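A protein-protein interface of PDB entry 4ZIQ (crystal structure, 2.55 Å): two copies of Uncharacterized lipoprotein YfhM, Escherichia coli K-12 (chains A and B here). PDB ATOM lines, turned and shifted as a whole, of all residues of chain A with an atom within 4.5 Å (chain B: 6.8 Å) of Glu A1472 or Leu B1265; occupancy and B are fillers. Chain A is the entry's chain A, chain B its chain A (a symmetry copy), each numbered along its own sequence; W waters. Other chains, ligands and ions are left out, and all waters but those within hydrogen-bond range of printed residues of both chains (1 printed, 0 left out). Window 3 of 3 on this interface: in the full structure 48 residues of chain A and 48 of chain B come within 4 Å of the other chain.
The backbone NH (N) of Trp A1497 is in hydrogen-bond range of the backbone carbonyl oxygen (O) of His A1474 (2.8 Å).
O of Glu A1472 lies within hydrogen-bond range of N of Gln A1499 (2.9 Å).
Glu A1472 touches Leu B1265 (OE2 to CD2, 3.7 Å).
O of Gly B1255 touches NE2 of His A1474 (3.5 Å).
Trp A1497 touches Gly B1255 (CZ3 to O, 3.6 Å).
Trp A1497 touches Met B1257.
CZ2 of Trp A1497 touches OG of Ser B1258 (3.6 Å).
CA of Pro B1260 touches OE1 of Gln A1499 (3.8 Å).
Water W1 lies within hydrogen-bond range of OE1 of Gln A1499 (2.9 Å) and N of Ile B1259 (2.9 Å).
Glu A1472 touches one residue of chain B.
Of the printed residues of chain B, Trp A1497 touches Gly B1255, Met B1257 and Ser B1258.
Ile B1259 touches none of the printed residues of chain A.
Of the printed residues of chain A, Pro B1260 touches Gln A1499.
Asn B1264 touches none of the printed residues of chain A.
Of the printed residues of chain A, Leu B1265 touches Glu A1472 (3.7 Å).
Of the 16 printed residues of chain B, 5 touch a printed residue of chain A.
Among the printed residues, 6 pairs touch across the chains.
Among the printed residues, no Asp or Glu carboxylate lies within 4 Å of a Lys or Arg side-chain nitrogen of the other chain.
No position is printed for both chains.
Of the 6 pairs that touch across the chains among the printed residues, none has its exchanged pair printed and touching as well.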
ATOM      1  N   ILE A1471     -17.588  20.645  33.816  1.00  0.00           N
ATOM      2  CA  ILE A1471     -16.408  19.819  34.032  1.00  0.00           C
ATOM      3  C   ILE A1471     -16.123  18.991  32.786  1.00  0.00           C
ATOM      4  O   ILE A1471     -17.036  18.469  32.141  1.00  0.00           O
ATOM      5  CB  ILE A1471     -16.482  18.937  35.324  1.00  0.00           C
ATOM      6  CG1 ILE A1471     -15.073  18.338  35.693  1.00  0.00           C
ATOM      7  CG2 ILE A1471     -17.595  17.860  35.256  1.00  0.00           C
ATOM      8  CD1 ILE A1471     -14.897  17.858  37.088  1.00  0.00           C
ATOM      9  N   GLU A1472     -14.843  18.885  32.453  1.00  0.00           N
ATOM     10  CA  GLU A1472     -14.366  18.069  31.353  1.00  0.00           C
ATOM     11  C   GLU A1472     -13.077  17.409  31.784  1.00  0.00           C
ATOM     12  O   GLU A1472     -12.299  17.969  32.572  1.00  0.00           O
ATOM     13  CB  GLU A1472     -14.235  18.847  30.029  1.00  0.00           C
ATOM     14  CG  GLU A1472     -13.230  19.987  29.997  1.00  0.00           C
ATOM     15  CD  GLU A1472     -13.044  20.596  28.617  1.00  0.00           C
ATOM     16  OE1 GLU A1472     -12.125  20.156  27.879  1.00  0.00           O
ATOM     17  OE2 GLU A1472     -13.836  21.502  28.267  1.00  0.00           O
ATOM     18  N   ARG A1473     -12.926  16.163  31.353  1.00  0.00           N
ATOM     19  CA  ARG A1473     -11.762  15.326  31.626  1.00  0.00           C
ATOM     20  C   ARG A1473     -11.078  14.911  30.333  1.00  0.00           C
ATOM     21  O   ARG A1473     -11.730  14.609  29.325  1.00  0.00           O
ATOM     22  CB  ARG A1473     -12.171  14.084  32.426  1.00  0.00           C
ATOM     23  CG  ARG A1473     -10.993  13.353  33.024  1.00  0.00           C
ATOM     24  CD  ARG A1473     -11.242  11.871  33.134  1.00  0.00           C
ATOM     25  NE  ARG A1473     -12.107  11.552  34.260  1.00  0.00           N
ATOM     26  CZ  ARG A1473     -13.238  10.863  34.159  1.00  0.00           C
ATOM     27  NH1 ARG A1473     -13.644  10.409  32.978  1.00  0.00           N
ATOM     28  NH2 ARG A1473     -13.959  10.601  35.239  1.00  0.00           N
ATOM     29  N   HIS A1474      -9.758  14.867  30.380  1.00  0.00           N
ATOM     30  CA  HIS A1474      -8.928  14.413  29.272  1.00  0.00           C
ATOM     31  C   HIS A1474      -7.726  13.734  29.840  1.00  0.00           C
ATOM     32  O   HIS A1474      -7.191  14.186  30.850  1.00  0.00           O
ATOM     33  CB  HIS A1474      -8.532  15.566  28.348  1.00  0.00           C
ATOM     34  CG  HIS A1474      -8.049  15.090  27.025  1.00  0.00           C
ATOM     35  ND1 HIS A1474      -8.929  14.635  26.058  1.00  0.00           N
ATOM     36  CD2 HIS A1474      -6.787  14.973  26.558  1.00  0.00           C
ATOM     37  CE1 HIS A1474      -8.175  14.285  25.024  1.00  0.00           C
ATOM     38  NE2 HIS A1474      -6.881  14.460  25.287  1.00  0.00           N
ATOM     39  N   TRP A1497      -6.231  15.188  33.251  1.00  0.00           N
ATOM     40  CA  TRP A1497      -6.460  16.616  33.215  1.00  0.00           C
ATOM     41  C   TRP A1497      -7.963  16.952  33.329  1.00  0.00           C
ATOM     42  O   TRP A1497      -8.780  16.545  32.494  1.00  0.00           O
ATOM     43  CB  TRP A1497      -5.820  17.159  31.927  1.00  0.00           C
ATOM     44  CG  TRP A1497      -6.236  18.530  31.479  1.00  0.00           C
ATOM     45  CD1 TRP A1497      -6.598  19.590  32.261  1.00  0.00           C
ATOM     46  CD2 TRP A1497      -6.247  19.005  30.125  1.00  0.00           C
ATOM     47  NE1 TRP A1497      -6.897  20.678  31.471  1.00  0.00           N
ATOM     48  CE2 TRP A1497      -6.693  20.345  30.155  1.00  0.00           C
ATOM     49  CE3 TRP A1497      -5.971  18.405  28.875  1.00  0.00           C
ATOM     50  CZ2 TRP A1497      -6.832  21.114  28.993  1.00  0.00           C
ATOM     51  CZ3 TRP A1497      -6.112  19.167  27.720  1.00  0.00           C
ATOM     52  CH2 TRP A1497      -6.509  20.510  27.787  1.00  0.00           C
ATOM     53  N   LEU A1498      -8.303  17.707  34.372  1.00  0.00           N
ATOM     54  CA  LEU A1498      -9.673  18.184  34.620  1.00  0.00           C
ATOM     55  C   LEU A1498      -9.758  19.672  34.435  1.00  0.00           C
ATOM     56  O   LEU A1498      -8.862  20.389  34.882  1.00  0.00           O
ATOM     57  CB  LEU A1498     -10.156  17.840  36.045  1.00  0.00           C
ATOM     58  CG  LEU A1498     -10.238  16.346  36.408  1.00  0.00           C
ATOM     59  CD1 LEU A1498     -10.144  16.155  37.918  1.00  0.00           C
ATOM     60  CD2 LEU A1498     -11.499  15.713  35.843  1.00  0.00           C
ATOM     61  N   GLN A1499     -10.817  20.140  33.770  1.00  0.00           N
ATOM     62  CA  GLN A1499     -11.063  21.572  33.631  1.00  0.00           C
ATOM     63  C   GLN A1499     -12.453  21.860  34.129  1.00  0.00           C
ATOM     64  O   GLN A1499     -13.407  21.240  33.678  1.00  0.00           O
ATOM     65  CB  GLN A1499     -10.862  22.105  32.204  1.00  0.00           C
ATOM     66  CG  GLN A1499     -10.761  23.632  32.213  1.00  0.00           C
ATOM     67  CD  GLN A1499     -10.891  24.247  30.857  1.00  0.00           C
ATOM     68  OE1 GLN A1499     -10.021  24.095  29.984  1.00  0.00           O
ATOM     69  NE2 GLN A1499     -11.945  25.033  30.683  1.00  0.00           N
ATOM     70  N   GLY B1255      -7.310  17.575  20.943  1.00  0.00           N
ATOM     71  CA  GLY B1255      -7.612  17.229  22.326  1.00  0.00           C
ATOM     72  C   GLY B1255      -6.608  17.703  23.353  1.00  0.00           C
ATOM     73  O   GLY B1255      -6.969  17.893  24.511  1.00  0.00           O
ATOM     74  N   MET B1257      -5.190  20.624  23.324  1.00  0.00           N
ATOM     75  CA  MET B1257      -5.234  22.086  23.338  1.00  0.00           C
ATOM     76  C   MET B1257      -5.942  22.625  24.588  1.00  0.00           C
ATOM     77  O   MET B1257      -7.115  22.313  24.837  1.00  0.00           O
ATOM     78  CB  MET B1257      -5.897  22.651  22.063  1.00  0.00           C
ATOM     79  CG  MET B1257      -5.050  22.518  20.819  1.00  0.00           C
ATOM     80  SD  MET B1257      -5.842  23.225  19.337  1.00  0.00           S
ATOM     81  CE  MET B1257      -5.059  22.287  18.112  1.00  0.00           C
ATOM     82  N   SER B1258      -5.223  23.455  25.366  1.00  0.00           N
ATOM     83  CA  SER B1258      -5.787  24.086  26.566  1.00  0.00           C
ATOM     84  C   SER B1258      -6.086  25.559  26.275  1.00  0.00           C
ATOM     85  O   SER B1258      -5.164  26.378  26.165  1.00  0.00           O
ATOM     86  CB  SER B1258      -4.847  23.942  27.759  1.00  0.00           C
ATOM     87  OG  SER B1258      -5.464  24.442  28.931  1.00  0.00           O
ATOM     88  N   ILE B1259      -7.366  25.879  26.068  1.00  0.00           N
ATOM     89  CA  ILE B1259      -7.801  27.260  25.791  1.00  0.00           C
ATOM     90  C   ILE B1259      -8.885  27.541  26.840  1.00  0.00           C
ATOM     91  O   ILE B1259     -10.068  27.442  26.507  1.00  0.00           O
ATOM     92  CB  ILE B1259      -8.263  27.471  24.306  1.00  0.00           C
ATOM     93  CG1 ILE B1259      -7.338  26.772  23.278  1.00  0.00           C
ATOM     94  CG2 ILE B1259      -8.338  28.953  23.986  1.00  0.00           C
ATOM     95  CD1 ILE B1259      -8.040  26.276  21.947  1.00  0.00           C
ATOM     96  N   PRO B1260      -8.529  27.725  28.139  1.00  0.00           N
ATOM     97  CA  PRO B1260      -9.577  27.783  29.184  1.00  0.00           C
ATOM     98  C   PRO B1260     -10.509  28.995  29.144  1.00  0.00           C
ATOM     99  O   PRO B1260     -11.606  28.912  29.665  1.00  0.00           O
ATOM    100  CB  PRO B1260      -8.787  27.753  30.498  1.00  0.00           C
ATOM    101  CG  PRO B1260      -7.439  28.219  30.151  1.00  0.00           C
ATOM    102  CD  PRO B1260      -7.180  27.821  28.732  1.00  0.00           C
ATOM    103  N   ALA B1262     -11.843  30.271  26.421  1.00  0.00           N
ATOM    104  CA  ALA B1262     -12.657  30.185  25.215  1.00  0.00           C
ATOM    105  C   ALA B1262     -14.107  29.893  25.555  1.00  0.00           C
ATOM    106  O   ALA B1262     -14.390  28.950  26.289  1.00  0.00           O
ATOM    107  CB  ALA B1262     -12.097  29.125  24.267  1.00  0.00           C
ATOM    108  N   ASP B1263     -15.026  30.701  25.010  1.00  0.00           N
ATOM    109  CA  ASP B1263     -16.464  30.520  25.220  1.00  0.00           C
ATOM    110  C   ASP B1263     -16.975  29.336  24.391  1.00  0.00           C
ATOM    111  O   ASP B1263     -17.739  28.508  24.895  1.00  0.00           O
ATOM    112  CB  ASP B1263     -17.226  31.815  24.904  1.00  0.00           C
ATOM    113  CG  ASP B1263     -16.916  32.912  25.913  1.00  0.00           C
ATOM    114  OD1 ASP B1263     -17.361  32.789  27.084  1.00  0.00           O
ATOM    115  OD2 ASP B1263     -16.174  33.861  25.552  1.00  0.00           O
ATOM    116  N   ASN B1264     -16.504  29.234  23.144  1.00  0.00           N
ATOM    117  CA  ASN B1264     -16.827  28.150  22.231  1.00  0.00           C
ATOM    118  C   ASN B1264     -15.528  27.417  21.909  1.00  0.00           C
ATOM    119  O   ASN B1264     -14.889  27.719  20.896  1.00  0.00           O
ATOM    120  CB  ASN B1264     -17.518  28.705  20.978  1.00  0.00           C
ATOM    121  CG  ASN B1264     -18.336  27.700  20.213  1.00  0.00           C
ATOM    122  OD1 ASN B1264     -18.254  26.479  20.412  1.00  0.00           O
ATOM    123  ND2 ASN B1264     -19.103  28.201  19.266  1.00  0.00           N
ATOM    124  N   LEU B1265     -15.113  26.487  22.808  1.00  0.00           N
ATOM    125  CA  LEU B1265     -13.865  25.721  22.720  1.00  0.00           C
ATOM    126  C   LEU B1265     -13.698  24.967  21.382  1.00  0.00           C
ATOM    127  O   LEU B1265     -12.615  25.043  20.793  1.00  0.00           O
ATOM    128  CB  LEU B1265     -13.737  24.746  23.894  1.00  0.00           C
ATOM    129  CG  LEU B1265     -12.435  23.930  23.997  1.00  0.00           C
ATOM    130  CD1 LEU B1265     -11.184  24.830  24.052  1.00  0.00           C
ATOM    131  CD2 LEU B1265     -12.494  22.949  25.179  1.00  0.00           C
ATOM    132  N   LYS B1266     -14.753  24.262  20.905  1.00  0.00           N
ATOM    133  CA  LYS B1266     -14.726  23.512  19.652  1.00  0.00           C
ATOM    134  C   LYS B1266     -14.497  24.461  18.442  1.00  0.00           C
ATOM    135  O   LYS B1266     -13.735  24.114  17.539  1.00  0.00           O
ATOM    136  CB  LYS B1266     -15.986  22.637  19.474  1.00  0.00           C
ATOM    137  CG  LYS B1266     -17.320  23.388  19.489  1.00  0.00           C
ATOM    138  CD  LYS B1266     -18.466  22.558  18.920  1.00  0.00           C
ATOM    139  CE  LYS B1266     -19.748  23.346  18.803  1.00  0.00           C
ATOM    140  NZ  LYS B1266     -20.713  22.678  17.888  1.00  0.00           N
ATOM    141  N   ALA B1267     -15.108  25.668  18.464  1.00  0.00           N
ATOM    142  CA  ALA B1267     -14.969  26.700  17.422  1.00  0.00           C
ATOM    143  C   ALA B1267     -13.548  27.239  17.401  1.00  0.00           C
ATOM    144  O   ALA B1267     -12.992  27.442  16.321  1.00  0.00           O
ATOM    145  CB  ALA B1267     -15.965  27.833  17.653  1.00  0.00           C
ATOM    146  N   SER B1268     -12.958  27.445  18.600  1.00  0.00           N
ATOM    147  CA  SER B1268     -11.581  27.907  18.776  1.00  0.00           C
ATOM    148  C   SER B1268     -10.623  26.870  18.235  1.00  0.00           C
ATOM    149  O   SER B1268      -9.824  27.187  17.354  1.00  0.00           O
ATOM    150  CB  SER B1268     -11.309  28.188  20.243  1.00  0.00           C
ATOM    151  OG  SER B1268     -12.204  29.215  20.614  1.00  0.00           O
ATOM    152  N   LYS B1269     -10.786  25.611  18.675  1.00  0.00           N
ATOM    153  CA  LYS B1269     -10.003  24.460  18.229  1.00  0.00           C
ATOM    154  C   LYS B1269     -10.096  24.299  16.721  1.00  0.00           C
ATOM    155  O   LYS B1269      -9.064  24.081  16.097  1.00  0.00           O
ATOM    156  CB  LYS B1269     -10.460  23.179  18.940  1.00  0.00           C
ATOM    157  CG  LYS B1269      -9.930  23.060  20.360  1.00  0.00           C
ATOM    158  CD  LYS B1269     -10.216  21.706  20.965  1.00  0.00           C
ATOM    159  CE  LYS B1269      -9.793  21.696  22.419  1.00  0.00           C
ATOM    160  NZ  LYS B1269     -10.065  20.395  23.087  1.00  0.00           N
ATOM    161  N   PHE B1270     -11.296  24.503  16.128  1.00  0.00           N
ATOM    162  CA  PHE B1270     -11.517  24.393  14.686  1.00  0.00           C
ATOM    163  C   PHE B1270     -10.796  25.515  13.919  1.00  0.00           C
ATOM    164  O   PHE B1270     -10.214  25.232  12.867  1.00  0.00           O
ATOM    165  CB  PHE B1270     -13.034  24.368  14.334  1.00  0.00           C
ATOM    166  CG  PHE B1270     -13.320  24.016  12.882  1.00  0.00           C
ATOM    167  CD1 PHE B1270     -13.478  22.688  12.487  1.00  0.00           C
ATOM    168  CD2 PHE B1270     -13.400  25.008  11.909  1.00  0.00           C
ATOM    169  CE1 PHE B1270     -13.704  22.362  11.146  1.00  0.00           C
ATOM    170  CE2 PHE B1270     -13.630  24.681  10.571  1.00  0.00           C
ATOM    171  CZ  PHE B1270     -13.784  23.360  10.200  1.00  0.00           C
ATOM    172  N   TRP B1342     -12.220  35.416  23.353  1.00  0.00           N
ATOM    173  CA  TRP B1342     -13.619  34.995  23.215  1.00  0.00           C
ATOM    174  C   TRP B1342     -13.617  33.776  22.316  1.00  0.00           C
ATOM    175  O   TRP B1342     -13.950  32.666  22.742  1.00  0.00           O
ATOM    176  CB  TRP B1342     -14.498  36.127  22.652  1.00  0.00           C
ATOM    177  CG  TRP B1342     -15.950  35.988  23.005  1.00  0.00           C
ATOM    178  CD1 TRP B1342     -16.617  36.646  23.998  1.00  0.00           C
ATOM    179  CD2 TRP B1342     -16.909  35.114  22.388  1.00  0.00           C
ATOM    180  NE1 TRP B1342     -17.933  36.243  24.035  1.00  0.00           N
ATOM    181  CE2 TRP B1342     -18.141  35.304  23.056  1.00  0.00           C
ATOM    182  CE3 TRP B1342     -16.851  34.195  21.324  1.00  0.00           C
ATOM    183  CZ2 TRP B1342     -19.303  34.607  22.699  1.00  0.00           C
ATOM    184  CZ3 TRP B1342     -18.002  33.499  20.978  1.00  0.00           C
ATOM    185  CH2 TRP B1342     -19.209  33.707  21.661  1.00  0.00           C
ATOM    186  N   LEU B1343     -13.177  33.988  21.070  1.00  0.00           N
ATOM    187  CA  LEU B1343     -13.008  32.928  20.093  1.00  0.00           C
ATOM    188  C   LEU B1343     -11.520  32.570  20.014  1.00  0.00           C
ATOM    189  O   LEU B1343     -11.204  31.430  19.730  1.00  0.00           O
ATOM    190  CB  LEU B1343     -13.587  33.319  18.728  1.00  0.00           C
ATOM    191  CG  LEU B1343     -14.345  32.212  17.994  1.00  0.00           C
ATOM    192  CD1 LEU B1343     -15.568  31.737  18.789  1.00  0.00           C
ATOM    193  CD2 LEU B1343     -14.771  32.674  16.616  1.00  0.00           C
HETATM  194  O   HOH W   1      -9.401  24.092  27.146  1.00  0.00           O
